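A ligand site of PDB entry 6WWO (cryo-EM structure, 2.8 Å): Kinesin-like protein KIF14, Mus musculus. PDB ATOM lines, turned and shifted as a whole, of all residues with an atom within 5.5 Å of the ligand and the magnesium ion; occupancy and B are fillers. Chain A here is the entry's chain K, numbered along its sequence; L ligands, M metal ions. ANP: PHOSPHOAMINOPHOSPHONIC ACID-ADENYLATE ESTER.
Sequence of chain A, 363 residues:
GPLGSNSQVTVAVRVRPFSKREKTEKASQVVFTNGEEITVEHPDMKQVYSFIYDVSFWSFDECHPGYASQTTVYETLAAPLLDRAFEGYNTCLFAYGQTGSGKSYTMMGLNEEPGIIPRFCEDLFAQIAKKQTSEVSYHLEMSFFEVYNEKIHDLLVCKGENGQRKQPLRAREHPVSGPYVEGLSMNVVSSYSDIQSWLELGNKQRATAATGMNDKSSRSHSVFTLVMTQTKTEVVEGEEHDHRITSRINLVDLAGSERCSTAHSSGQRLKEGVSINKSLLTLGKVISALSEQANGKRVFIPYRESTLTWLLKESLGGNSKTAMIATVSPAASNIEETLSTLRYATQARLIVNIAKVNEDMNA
The magnesium ion is bound by the side-chain hydroxyl (OG) of Ser 104, at 2.0 Å.
The magnesium ion is bound by OG of Ser 218 (2.2 Å).
O1G of the ligand is bound to the magnesium ion, at 2.3 Å.
Arg 206 touches the magnesium ion.
Asp 253 touches the magnesium ion (OD2 to MG, 3.2 Å).
Leu 254 touches the magnesium ion (O to MG, 3.5 Å).
Of the 27 residues printed, 5 come within 4 Å of the magnesium ion.
The nearest printed residue that does not touch the magnesium ion is Lys 103 (4.6 Å).
NH2 of Arg 14 sits close to N6 of the ligand, at 3.3 Å.
Arg 16 touches the ligand.
Pro 17 touches the ligand (CD to N1, 3.7 Å).
Ser 59 touches the ligand.
Gln 98 touches the ligand (O to O1B, 3.7 Å).
CG2 of Thr 99 touches O2G of the ligand, at 3.2 Å.
Gly 100 touches the ligand (N to N3B, 3.5 Å).
Gly 102 touches the ligand (N to O3A, 3.5 Å).
Lys 216 touches the ligand (O to O2A, 3.6 Å).
Ser 217 touches the ligand.
N of Gly 256 touches O3G of the ligand (3.8 Å).
16 residues have an atom within 4 Å of the ligand: Arg 14, Arg 16, Pro 17, Ser 59, Gln 98, Thr 99, Gly 100, Gly 102, Lys 103, Ser 104, Tyr 105, Asn 214, Lys 216, Ser 217, Ser 218 and Gly 256.
The nearest printed residue that does not touch the ligand is Ala 255 (4.2 Å).
The side-chain hydroxyl of Thr 106 is in hydrogen-bond range of the backbone carbonyl oxygen of Gly 102 (3.1 Å).
The backbone carbonyl oxygen of Gly 100 sits at hydrogen-bond distance from the guanidinium group of Arg 16, 2.6 Å away.
OG of Ser 101 is in hydrogen-bond range of O of Gln 98 (2.7 Å).
The backbone NH (N) of Ser 104 sits at hydrogen-bond distance from the side-chain carboxylate (OD1) of Asp 253.
The side-chain amide nitrogen (NE2) of Gln 70 sits at hydrogen-bond distance from the backbone carbonyl oxygen (O) of Tyr 105 (2.7 Å).
OG of Ser 59 sits close to O of Val 15 (3.5 Å).
NH2 of Arg 206 sits at hydrogen-bond distance from O of Ser 220.
The guanidinium group (NH1) of Arg 206 lies within salt-bridge range of the side-chain carboxylate (OD2) of Asp 253 (2.8 Å).
An oxygen (O1A) of the ligand lies within hydrogen-bond range of the backbone NH of Tyr 105 (3.1 Å).
The backbone NH (N) of Ser 104 sits at hydrogen-bond distance from an oxygen (O1A) of the ligand.
O2A of the ligand is in hydrogen-bond range of ND2 of Asn 214 (3.1 Å).
The side-chain amino group (NZ) of Lys 103 is in salt-bridge range of an oxygen (O1B) of the ligand (2.9 Å).
The backbone NH of Ser 218 is in hydrogen-bond range of an oxygen (O2G) of the ligand (3.4 Å).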
ATOM      1  N   ARG A  14      -8.994 -13.192   6.155  1.00  0.00           N
ATOM      2  CA  ARG A  14      -7.836 -13.990   5.793  1.00  0.00           C
ATOM      3  C   ARG A  14      -8.287 -15.339   5.235  1.00  0.00           C
ATOM      4  O   ARG A  14      -9.111 -16.020   5.854  1.00  0.00           O
ATOM      5  CB  ARG A  14      -6.931 -14.183   7.002  1.00  0.00           C
ATOM      6  CG  ARG A  14      -5.699 -15.027   6.792  1.00  0.00           C
ATOM      7  CD  ARG A  14      -4.579 -14.561   7.712  1.00  0.00           C
ATOM      8  NE  ARG A  14      -3.641 -15.627   8.089  1.00  0.00           N
ATOM      9  CZ  ARG A  14      -2.422 -15.815   7.597  1.00  0.00           C
ATOM     10  NH1 ARG A  14      -1.911 -15.038   6.649  1.00  0.00           N
ATOM     11  NH2 ARG A  14      -1.696 -16.815   8.062  1.00  0.00           N
ATOM     12  N   VAL A  15      -7.737 -15.712   4.074  1.00  0.00           N
ATOM     13  CA  VAL A  15      -8.037 -16.998   3.450  1.00  0.00           C
ATOM     14  C   VAL A  15      -6.912 -17.974   3.713  1.00  0.00           C
ATOM     15  O   VAL A  15      -5.727 -17.627   3.715  1.00  0.00           O
ATOM     16  CB  VAL A  15      -8.306 -16.832   1.943  1.00  0.00           C
ATOM     17  CG1 VAL A  15      -9.369 -15.797   1.724  1.00  0.00           C
ATOM     18  CG2 VAL A  15      -7.053 -16.449   1.168  1.00  0.00           C
ATOM     19  N   ARG A  16      -7.214 -19.252   3.735  1.00  0.00           N
ATOM     20  CA  ARG A  16      -6.200 -20.311   3.991  1.00  0.00           C
ATOM     21  C   ARG A  16      -5.897 -21.086   2.689  1.00  0.00           C
ATOM     22  O   ARG A  16      -6.820 -21.206   1.871  1.00  0.00           O
ATOM     23  CB  ARG A  16      -6.802 -21.239   5.055  1.00  0.00           C
ATOM     24  CG  ARG A  16      -5.982 -22.484   5.360  1.00  0.00           C
ATOM     25  CD  ARG A  16      -6.644 -23.509   6.168  1.00  0.00           C
ATOM     26  NE  ARG A  16      -8.065 -23.584   5.820  1.00  0.00           N
ATOM     27  CZ  ARG A  16      -8.568 -24.359   4.875  1.00  0.00           C
ATOM     28  NH1 ARG A  16      -7.998 -24.383   3.684  1.00  0.00           N
ATOM     29  NH2 ARG A  16      -9.615 -25.109   5.138  1.00  0.00           N
ATOM     30  N   PRO A  17      -4.649 -21.598   2.466  1.00  0.00           N
ATOM     31  CA  PRO A  17      -4.559 -22.442   1.265  1.00  0.00           C
ATOM     32  C   PRO A  17      -5.324 -23.759   1.418  1.00  0.00           C
ATOM     33  O   PRO A  17      -5.380 -24.227   2.522  1.00  0.00           O
ATOM     34  CB  PRO A  17      -3.102 -22.852   1.177  1.00  0.00           C
ATOM     35  CG  PRO A  17      -2.749 -23.008   2.603  1.00  0.00           C
ATOM     36  CD  PRO A  17      -3.371 -21.758   3.178  1.00  0.00           C
ATOM     37  N   SER A  59      -3.315 -16.063   1.693  1.00  0.00           N
ATOM     38  CA  SER A  59      -2.359 -17.134   1.962  1.00  0.00           C
ATOM     39  C   SER A  59      -2.560 -18.345   1.053  1.00  0.00           C
ATOM     40  O   SER A  59      -2.117 -19.444   1.383  1.00  0.00           O
ATOM     41  CB  SER A  59      -2.449 -17.555   3.418  1.00  0.00           C
ATOM     42  OG  SER A  59      -2.493 -16.434   4.268  1.00  0.00           O
ATOM     43  N   GLN A  70       2.718 -14.767   8.062  1.00  0.00           N
ATOM     44  CA  GLN A  70       2.500 -14.663   9.489  1.00  0.00           C
ATOM     45  C   GLN A  70       3.120 -13.390  10.043  1.00  0.00           C
ATOM     46  O   GLN A  70       2.593 -12.792  10.991  1.00  0.00           O
ATOM     47  CB  GLN A  70       3.057 -15.891  10.213  1.00  0.00           C
ATOM     48  CG  GLN A  70       2.549 -17.223   9.691  1.00  0.00           C
ATOM     49  CD  GLN A  70       1.094 -17.462  10.018  1.00  0.00           C
ATOM     50  OE1 GLN A  70       0.212 -17.346   9.170  1.00  0.00           O
ATOM     51  NE2 GLN A  70       0.838 -17.800  11.273  1.00  0.00           N
ATOM     52  N   GLN A  98     -14.456 -21.238  11.204  1.00  0.00           N
ATOM     53  CA  GLN A  98     -14.970 -22.623  11.348  1.00  0.00           C
ATOM     54  C   GLN A  98     -13.789 -23.575  11.606  1.00  0.00           C
ATOM     55  O   GLN A  98     -12.660 -23.106  11.600  1.00  0.00           O
ATOM     56  CB  GLN A  98     -15.754 -23.037  10.112  1.00  0.00           C
ATOM     57  CG  GLN A  98     -14.885 -23.422   8.922  1.00  0.00           C
ATOM     58  CD  GLN A  98     -15.696 -24.032   7.816  1.00  0.00           C
ATOM     59  OE1 GLN A  98     -15.913 -23.424   6.776  1.00  0.00           O
ATOM     60  NE2 GLN A  98     -16.183 -25.236   8.047  1.00  0.00           N
ATOM     61  N   THR A  99     -14.067 -24.831  11.840  1.00  0.00           N
ATOM     62  CA  THR A  99     -13.011 -25.835  12.103  1.00  0.00           C
ATOM     63  C   THR A  99     -12.153 -26.016  10.850  1.00  0.00           C
ATOM     64  O   THR A  99     -12.733 -26.372   9.827  1.00  0.00           O
ATOM     65  CB  THR A  99     -13.631 -27.144  12.580  1.00  0.00           C
ATOM     66  OG1 THR A  99     -14.845 -27.349  11.879  1.00  0.00           O
ATOM     67  CG2 THR A  99     -13.901 -27.133  14.066  1.00  0.00           C
ATOM     68  N   GLY A 100     -10.855 -25.767  10.897  1.00  0.00           N
ATOM     69  CA  GLY A 100      -9.973 -25.916   9.736  1.00  0.00           C
ATOM     70  C   GLY A 100      -9.730 -24.596   9.031  1.00  0.00           C
ATOM     71  O   GLY A 100      -9.000 -24.605   8.053  1.00  0.00           O
ATOM     72  N   SER A 101     -10.305 -23.502   9.499  1.00  0.00           N
ATOM     73  CA  SER A 101     -10.187 -22.190   8.881  1.00  0.00           C
ATOM     74  C   SER A 101      -8.922 -21.454   9.288  1.00  0.00           C
ATOM     75  O   SER A 101      -8.620 -20.407   8.702  1.00  0.00           O
ATOM     76  CB  SER A 101     -11.413 -21.329   9.223  1.00  0.00           C
ATOM     77  OG  SER A 101     -11.421 -20.972  10.598  1.00  0.00           O
ATOM     78  N   GLY A 102      -8.159 -21.968  10.240  1.00  0.00           N
ATOM     79  CA  GLY A 102      -6.853 -21.413  10.538  1.00  0.00           C
ATOM     80  C   GLY A 102      -6.834 -20.213  11.459  1.00  0.00           C
ATOM     81  O   GLY A 102      -6.361 -19.134  11.058  1.00  0.00           O
ATOM     82  N   LYS A 103      -7.319 -20.372  12.684  1.00  0.00           N
ATOM     83  CA  LYS A 103      -7.174 -19.364  13.720  1.00  0.00           C
ATOM     84  C   LYS A 103      -6.161 -19.739  14.788  1.00  0.00           C
ATOM     85  O   LYS A 103      -5.497 -18.863  15.334  1.00  0.00           O
ATOM     86  CB  LYS A 103      -8.514 -19.080  14.403  1.00  0.00           C
ATOM     87  CG  LYS A 103      -9.146 -20.262  15.075  1.00  0.00           C
ATOM     88  CD  LYS A 103     -10.556 -19.947  15.473  1.00  0.00           C
ATOM     89  CE  LYS A 103     -11.504 -20.360  14.390  1.00  0.00           C
ATOM     90  NZ  LYS A 103     -11.732 -21.810  14.497  1.00  0.00           N
ATOM     91  N   SER A 104      -6.029 -21.029  15.103  1.00  0.00           N
ATOM     92  CA  SER A 104      -4.993 -21.497  16.006  1.00  0.00           C
ATOM     93  C   SER A 104      -3.624 -21.603  15.325  1.00  0.00           C
ATOM     94  O   SER A 104      -2.651 -21.986  15.978  1.00  0.00           O
ATOM     95  CB  SER A 104      -5.381 -22.856  16.588  1.00  0.00           C
ATOM     96  OG  SER A 104      -6.662 -22.814  17.190  1.00  0.00           O
ATOM     97  N   TYR A 105      -3.541 -21.275  14.038  1.00  0.00           N
ATOM     98  CA  TYR A 105      -2.291 -21.133  13.319  1.00  0.00           C
ATOM     99  C   TYR A 105      -1.886 -19.685  13.120  1.00  0.00           C
ATOM    100  O   TYR A 105      -0.713 -19.414  12.861  1.00  0.00           O
ATOM    101  CB  TYR A 105      -2.375 -21.822  11.949  1.00  0.00           C
ATOM    102  CG  TYR A 105      -1.086 -21.835  11.177  1.00  0.00           C
ATOM    103  CD1 TYR A 105      -0.120 -22.798  11.399  1.00  0.00           C
ATOM    104  CD2 TYR A 105      -0.824 -20.870  10.210  1.00  0.00           C
ATOM    105  CE1 TYR A 105       1.069 -22.806  10.696  1.00  0.00           C
ATOM    106  CE2 TYR A 105       0.350 -20.862   9.504  1.00  0.00           C
ATOM    107  CZ  TYR A 105       1.292 -21.837   9.744  1.00  0.00           C
ATOM    108  OH  TYR A 105       2.472 -21.844   9.053  1.00  0.00           O
ATOM    109  N   THR A 106      -2.825 -18.753  13.222  1.00  0.00           N
ATOM    110  CA  THR A 106      -2.527 -17.339  13.115  1.00  0.00           C
ATOM    111  C   THR A 106      -2.086 -16.721  14.439  1.00  0.00           C
ATOM    112  O   THR A 106      -1.015 -16.101  14.490  1.00  0.00           O
ATOM    113  CB  THR A 106      -3.748 -16.584  12.608  1.00  0.00           C
ATOM    114  OG1 THR A 106      -4.087 -17.065  11.298  1.00  0.00           O
ATOM    115  CG2 THR A 106      -3.463 -15.122  12.531  1.00  0.00           C
ATOM    116  N   LEU A 110       2.956 -22.014  14.594  1.00  0.00           N
ATOM    117  CA  LEU A 110       3.579 -23.296  14.869  1.00  0.00           C
ATOM    118  C   LEU A 110       5.022 -23.035  15.291  1.00  0.00           C
ATOM    119  O   LEU A 110       5.449 -21.885  15.343  1.00  0.00           O
ATOM    120  CB  LEU A 110       3.497 -24.202  13.641  1.00  0.00           C
ATOM    121  CG  LEU A 110       2.181 -24.944  13.372  1.00  0.00           C
ATOM    122  CD1 LEU A 110       2.302 -25.769  12.096  1.00  0.00           C
ATOM    123  CD2 LEU A 110       1.770 -25.842  14.523  1.00  0.00           C
ATOM    124  N   ARG A 206      -4.613 -27.366  26.963  1.00  0.00           N
ATOM    125  CA  ARG A 206      -5.809 -27.024  26.212  1.00  0.00           C
ATOM    126  C   ARG A 206      -6.404 -28.263  25.568  1.00  0.00           C
ATOM    127  O   ARG A 206      -5.717 -29.016  24.877  1.00  0.00           O
ATOM    128  CB  ARG A 206      -5.470 -25.983  25.144  1.00  0.00           C
ATOM    129  CG  ARG A 206      -6.623 -25.637  24.214  1.00  0.00           C
ATOM    130  CD  ARG A 206      -6.418 -24.309  23.534  1.00  0.00           C
ATOM    131  NE  ARG A 206      -7.635 -23.864  22.870  1.00  0.00           N
ATOM    132  CZ  ARG A 206      -7.687 -22.962  21.890  1.00  0.00           C
ATOM    133  NH1 ARG A 206      -6.588 -22.366  21.444  1.00  0.00           N
ATOM    134  NH2 ARG A 206      -8.860 -22.638  21.364  1.00  0.00           N
ATOM    135  N   ASN A 214      -9.879 -31.461  11.043  1.00  0.00           N
ATOM    136  CA  ASN A 214      -8.401 -31.315  11.018  1.00  0.00           C
ATOM    137  C   ASN A 214      -7.768 -32.203  12.090  1.00  0.00           C
ATOM    138  O   ASN A 214      -8.428 -32.453  13.107  1.00  0.00           O
ATOM    139  CB  ASN A 214      -7.958 -29.857  11.128  1.00  0.00           C
ATOM    140  CG  ASN A 214      -8.268 -29.263  12.478  1.00  0.00           C
ATOM    141  OD1 ASN A 214      -9.406 -29.323  12.929  1.00  0.00           O
ATOM    142  ND2 ASN A 214      -7.267 -28.708  13.134  1.00  0.00           N
ATOM    143  N   LYS A 216      -5.386 -31.797  14.521  1.00  0.00           N
ATOM    144  CA  LYS A 216      -5.392 -31.315  15.920  1.00  0.00           C
ATOM    145  C   LYS A 216      -6.435 -30.205  15.993  1.00  0.00           C
ATOM    146  O   LYS A 216      -6.104 -29.072  15.609  1.00  0.00           O
ATOM    147  CB  LYS A 216      -4.005 -30.825  16.332  1.00  0.00           C
ATOM    148  CG  LYS A 216      -3.159 -31.872  17.057  1.00  0.00           C
ATOM    149  CD  LYS A 216      -1.753 -31.411  17.348  1.00  0.00           C
ATOM    150  CE  LYS A 216      -1.181 -30.519  16.257  1.00  0.00           C
ATOM    151  NZ  LYS A 216      -1.373 -31.101  14.913  1.00  0.00           N
ATOM    152  N   SER A 217      -7.621 -30.498  16.494  1.00  0.00           N
ATOM    153  CA  SER A 217      -8.735 -29.516  16.513  1.00  0.00           C
ATOM    154  C   SER A 217      -8.970 -29.052  17.945  1.00  0.00           C
ATOM    155  O   SER A 217      -9.171 -29.925  18.798  1.00  0.00           O
ATOM    156  CB  SER A 217      -9.974 -30.138  15.992  1.00  0.00           C
ATOM    157  OG  SER A 217     -10.564 -30.956  16.977  1.00  0.00           O
ATOM    158  N   SER A 218      -8.976 -27.756  18.191  1.00  0.00           N
ATOM    159  CA  SER A 218      -9.193 -27.240  19.561  1.00  0.00           C
ATOM    160  C   SER A 218     -10.676 -27.415  19.914  1.00  0.00           C
ATOM    161  O   SER A 218     -11.503 -27.089  19.075  1.00  0.00           O
ATOM    162  CB  SER A 218      -8.796 -25.817  19.626  1.00  0.00           C
ATOM    163  OG  SER A 218      -9.747 -25.027  18.957  1.00  0.00           O
ATOM    164  N   ARG A 219     -11.014 -27.874  21.115  1.00  0.00           N
ATOM    165  CA  ARG A 219     -12.409 -28.076  21.558  1.00  0.00           C
ATOM    166  C   ARG A 219     -12.721 -27.100  22.669  1.00  0.00           C
ATOM    167  O   ARG A 219     -13.535 -27.432  23.536  1.00  0.00           O
ATOM    168  CB  ARG A 219     -12.469 -29.504  22.055  1.00  0.00           C
ATOM    169  CG  ARG A 219     -11.718 -30.486  21.171  1.00  0.00           C
ATOM    170  CD  ARG A 219     -12.365 -30.621  19.812  1.00  0.00           C
ATOM    171  NE  ARG A 219     -13.728 -31.112  19.917  1.00  0.00           N
ATOM    172  CZ  ARG A 219     -14.623 -30.995  18.965  1.00  0.00           C
ATOM    173  NH1 ARG A 219     -14.371 -30.237  17.917  1.00  0.00           N
ATOM    174  NH2 ARG A 219     -15.763 -31.649  19.043  1.00  0.00           N
ATOM    175  N   SER A 220     -12.018 -25.964  22.690  1.00  0.00           N
ATOM    176  CA  SER A 220     -12.036 -24.988  23.763  1.00  0.00           C
ATOM    177  C   SER A 220     -11.811 -23.609  23.169  1.00  0.00           C
ATOM    178  O   SER A 220     -11.233 -23.480  22.098  1.00  0.00           O
ATOM    179  CB  SER A 220     -10.941 -25.288  24.794  1.00  0.00           C
ATOM    180  OG  SER A 220     -11.006 -26.630  25.254  1.00  0.00           O
ATOM    181  N   ASP A 253      -8.260 -17.172  21.253  1.00  0.00           N
ATOM    182  CA  ASP A 253      -8.303 -18.129  20.153  1.00  0.00           C
ATOM    183  C   ASP A 253      -9.513 -19.034  20.396  1.00  0.00           C
ATOM    184  O   ASP A 253      -9.534 -19.799  21.356  1.00  0.00           O
ATOM    185  CB  ASP A 253      -7.024 -18.931  20.049  1.00  0.00           C
ATOM    186  CG  ASP A 253      -7.008 -19.863  18.867  1.00  0.00           C
ATOM    187  OD1 ASP A 253      -6.815 -19.379  17.735  1.00  0.00           O
ATOM    188  OD2 ASP A 253      -7.197 -21.074  19.071  1.00  0.00           O
ATOM    189  N   LEU A 254     -10.495 -18.930  19.516  1.00  0.00           N
ATOM    190  CA  LEU A 254     -11.774 -19.574  19.720  1.00  0.00           C
ATOM    191  C   LEU A 254     -11.775 -20.981  19.117  1.00  0.00           C
ATOM    192  O   LEU A 254     -10.795 -21.448  18.530  1.00  0.00           O
ATOM    193  CB  LEU A 254     -12.886 -18.730  19.124  1.00  0.00           C
ATOM    194  CG  LEU A 254     -13.017 -17.312  19.660  1.00  0.00           C
ATOM    195  CD1 LEU A 254     -14.150 -16.613  18.986  1.00  0.00           C
ATOM    196  CD2 LEU A 254     -13.218 -17.282  21.150  1.00  0.00           C
ATOM    197  N   ALA A 255     -12.895 -21.667  19.297  1.00  0.00           N
ATOM    198  CA  ALA A 255     -13.180 -22.954  18.692  1.00  0.00           C
ATOM    199  C   ALA A 255     -14.044 -22.749  17.451  1.00  0.00           C
ATOM    200  O   ALA A 255     -14.241 -21.624  16.987  1.00  0.00           O
ATOM    201  CB  ALA A 255     -13.826 -23.859  19.724  1.00  0.00           C
ATOM    202  N   GLY A 256     -14.554 -23.800  16.787  1.00  0.00           N
ATOM    203  CA  GLY A 256     -15.237 -23.563  15.496  1.00  0.00           C
ATOM    204  C   GLY A 256     -16.631 -24.145  15.338  1.00  0.00           C
ATOM    205  O   GLY A 256     -16.974 -25.091  16.057  1.00  0.00           O
HETATM  206  PG  ANP L   1     -10.430 -25.716  15.400  1.00  0.00           P
HETATM  207  O1G ANP L   1      -9.470 -25.298  16.448  1.00  0.00           O
HETATM  208  O2G ANP L   1     -11.088 -27.021  15.617  1.00  0.00           O
HETATM  209  O3G ANP L   1     -11.319 -24.629  14.935  1.00  0.00           O
HETATM  210  PB  ANP L   1      -8.533 -24.512  13.790  1.00  0.00           P
HETATM  211  O1B ANP L   1      -9.520 -23.406  13.600  1.00  0.00           O
HETATM  212  O2B ANP L   1      -7.607 -24.462  14.928  1.00  0.00           O
HETATM  213  N3B ANP L   1      -9.412 -25.938  14.082  1.00  0.00           N
HETATM  214  PA  ANP L   1      -6.077 -24.817  12.813  1.00  0.00           P
HETATM  215  O1A ANP L   1      -5.510 -23.529  13.233  1.00  0.00           O
HETATM  216  O2A ANP L   1      -5.969 -25.994  13.712  1.00  0.00           O
HETATM  217  O3A ANP L   1      -7.601 -24.614  12.521  1.00  0.00           O
HETATM  218  O5' ANP L   1      -5.441 -25.119  11.402  1.00  0.00           O
HETATM  219  C5' ANP L   1      -5.713 -26.301  10.666  1.00  0.00           C
HETATM  220  C4' ANP L   1      -4.531 -26.570   9.760  1.00  0.00           C
HETATM  221  O4' ANP L   1      -4.515 -25.617   8.709  1.00  0.00           O
HETATM  222  C3' ANP L   1      -3.231 -26.426  10.509  1.00  0.00           C
HETATM  223  O3' ANP L   1      -2.530 -27.664  10.522  1.00  0.00           O
HETATM  224  C2' ANP L   1      -2.466 -25.339   9.791  1.00  0.00           C
HETATM  225  O2' ANP L   1      -1.113 -25.685   9.530  1.00  0.00           O
HETATM  226  C1' ANP L   1      -3.191 -25.169   8.486  1.00  0.00           C
HETATM  227  N9  ANP L   1      -3.188 -23.760   8.132  1.00  0.00           N
HETATM  228  C8  ANP L   1      -4.075 -22.872   8.569  1.00  0.00           C
HETATM  229  N7  ANP L   1      -3.807 -21.661   8.064  1.00  0.00           N
HETATM  230  C5  ANP L   1      -2.725 -21.776   7.306  1.00  0.00           C
HETATM  231  C6  ANP L   1      -1.941 -20.863   6.482  1.00  0.00           C
HETATM  232  N6  ANP L   1      -2.296 -19.582   6.419  1.00  0.00           N
HETATM  233  N1  ANP L   1      -0.889 -21.352   5.827  1.00  0.00           N
HETATM  234  C2  ANP L   1      -0.548 -22.643   5.906  1.00  0.00           C
HETATM  235  N3  ANP L   1      -1.242 -23.535   6.645  1.00  0.00           N
HETATM  236  C4  ANP L   1      -2.325 -23.159   7.341  1.00  0.00           C
HETATM  237 MG    MG M   1      -8.278 -23.828  17.801  1.00  0.00          MG
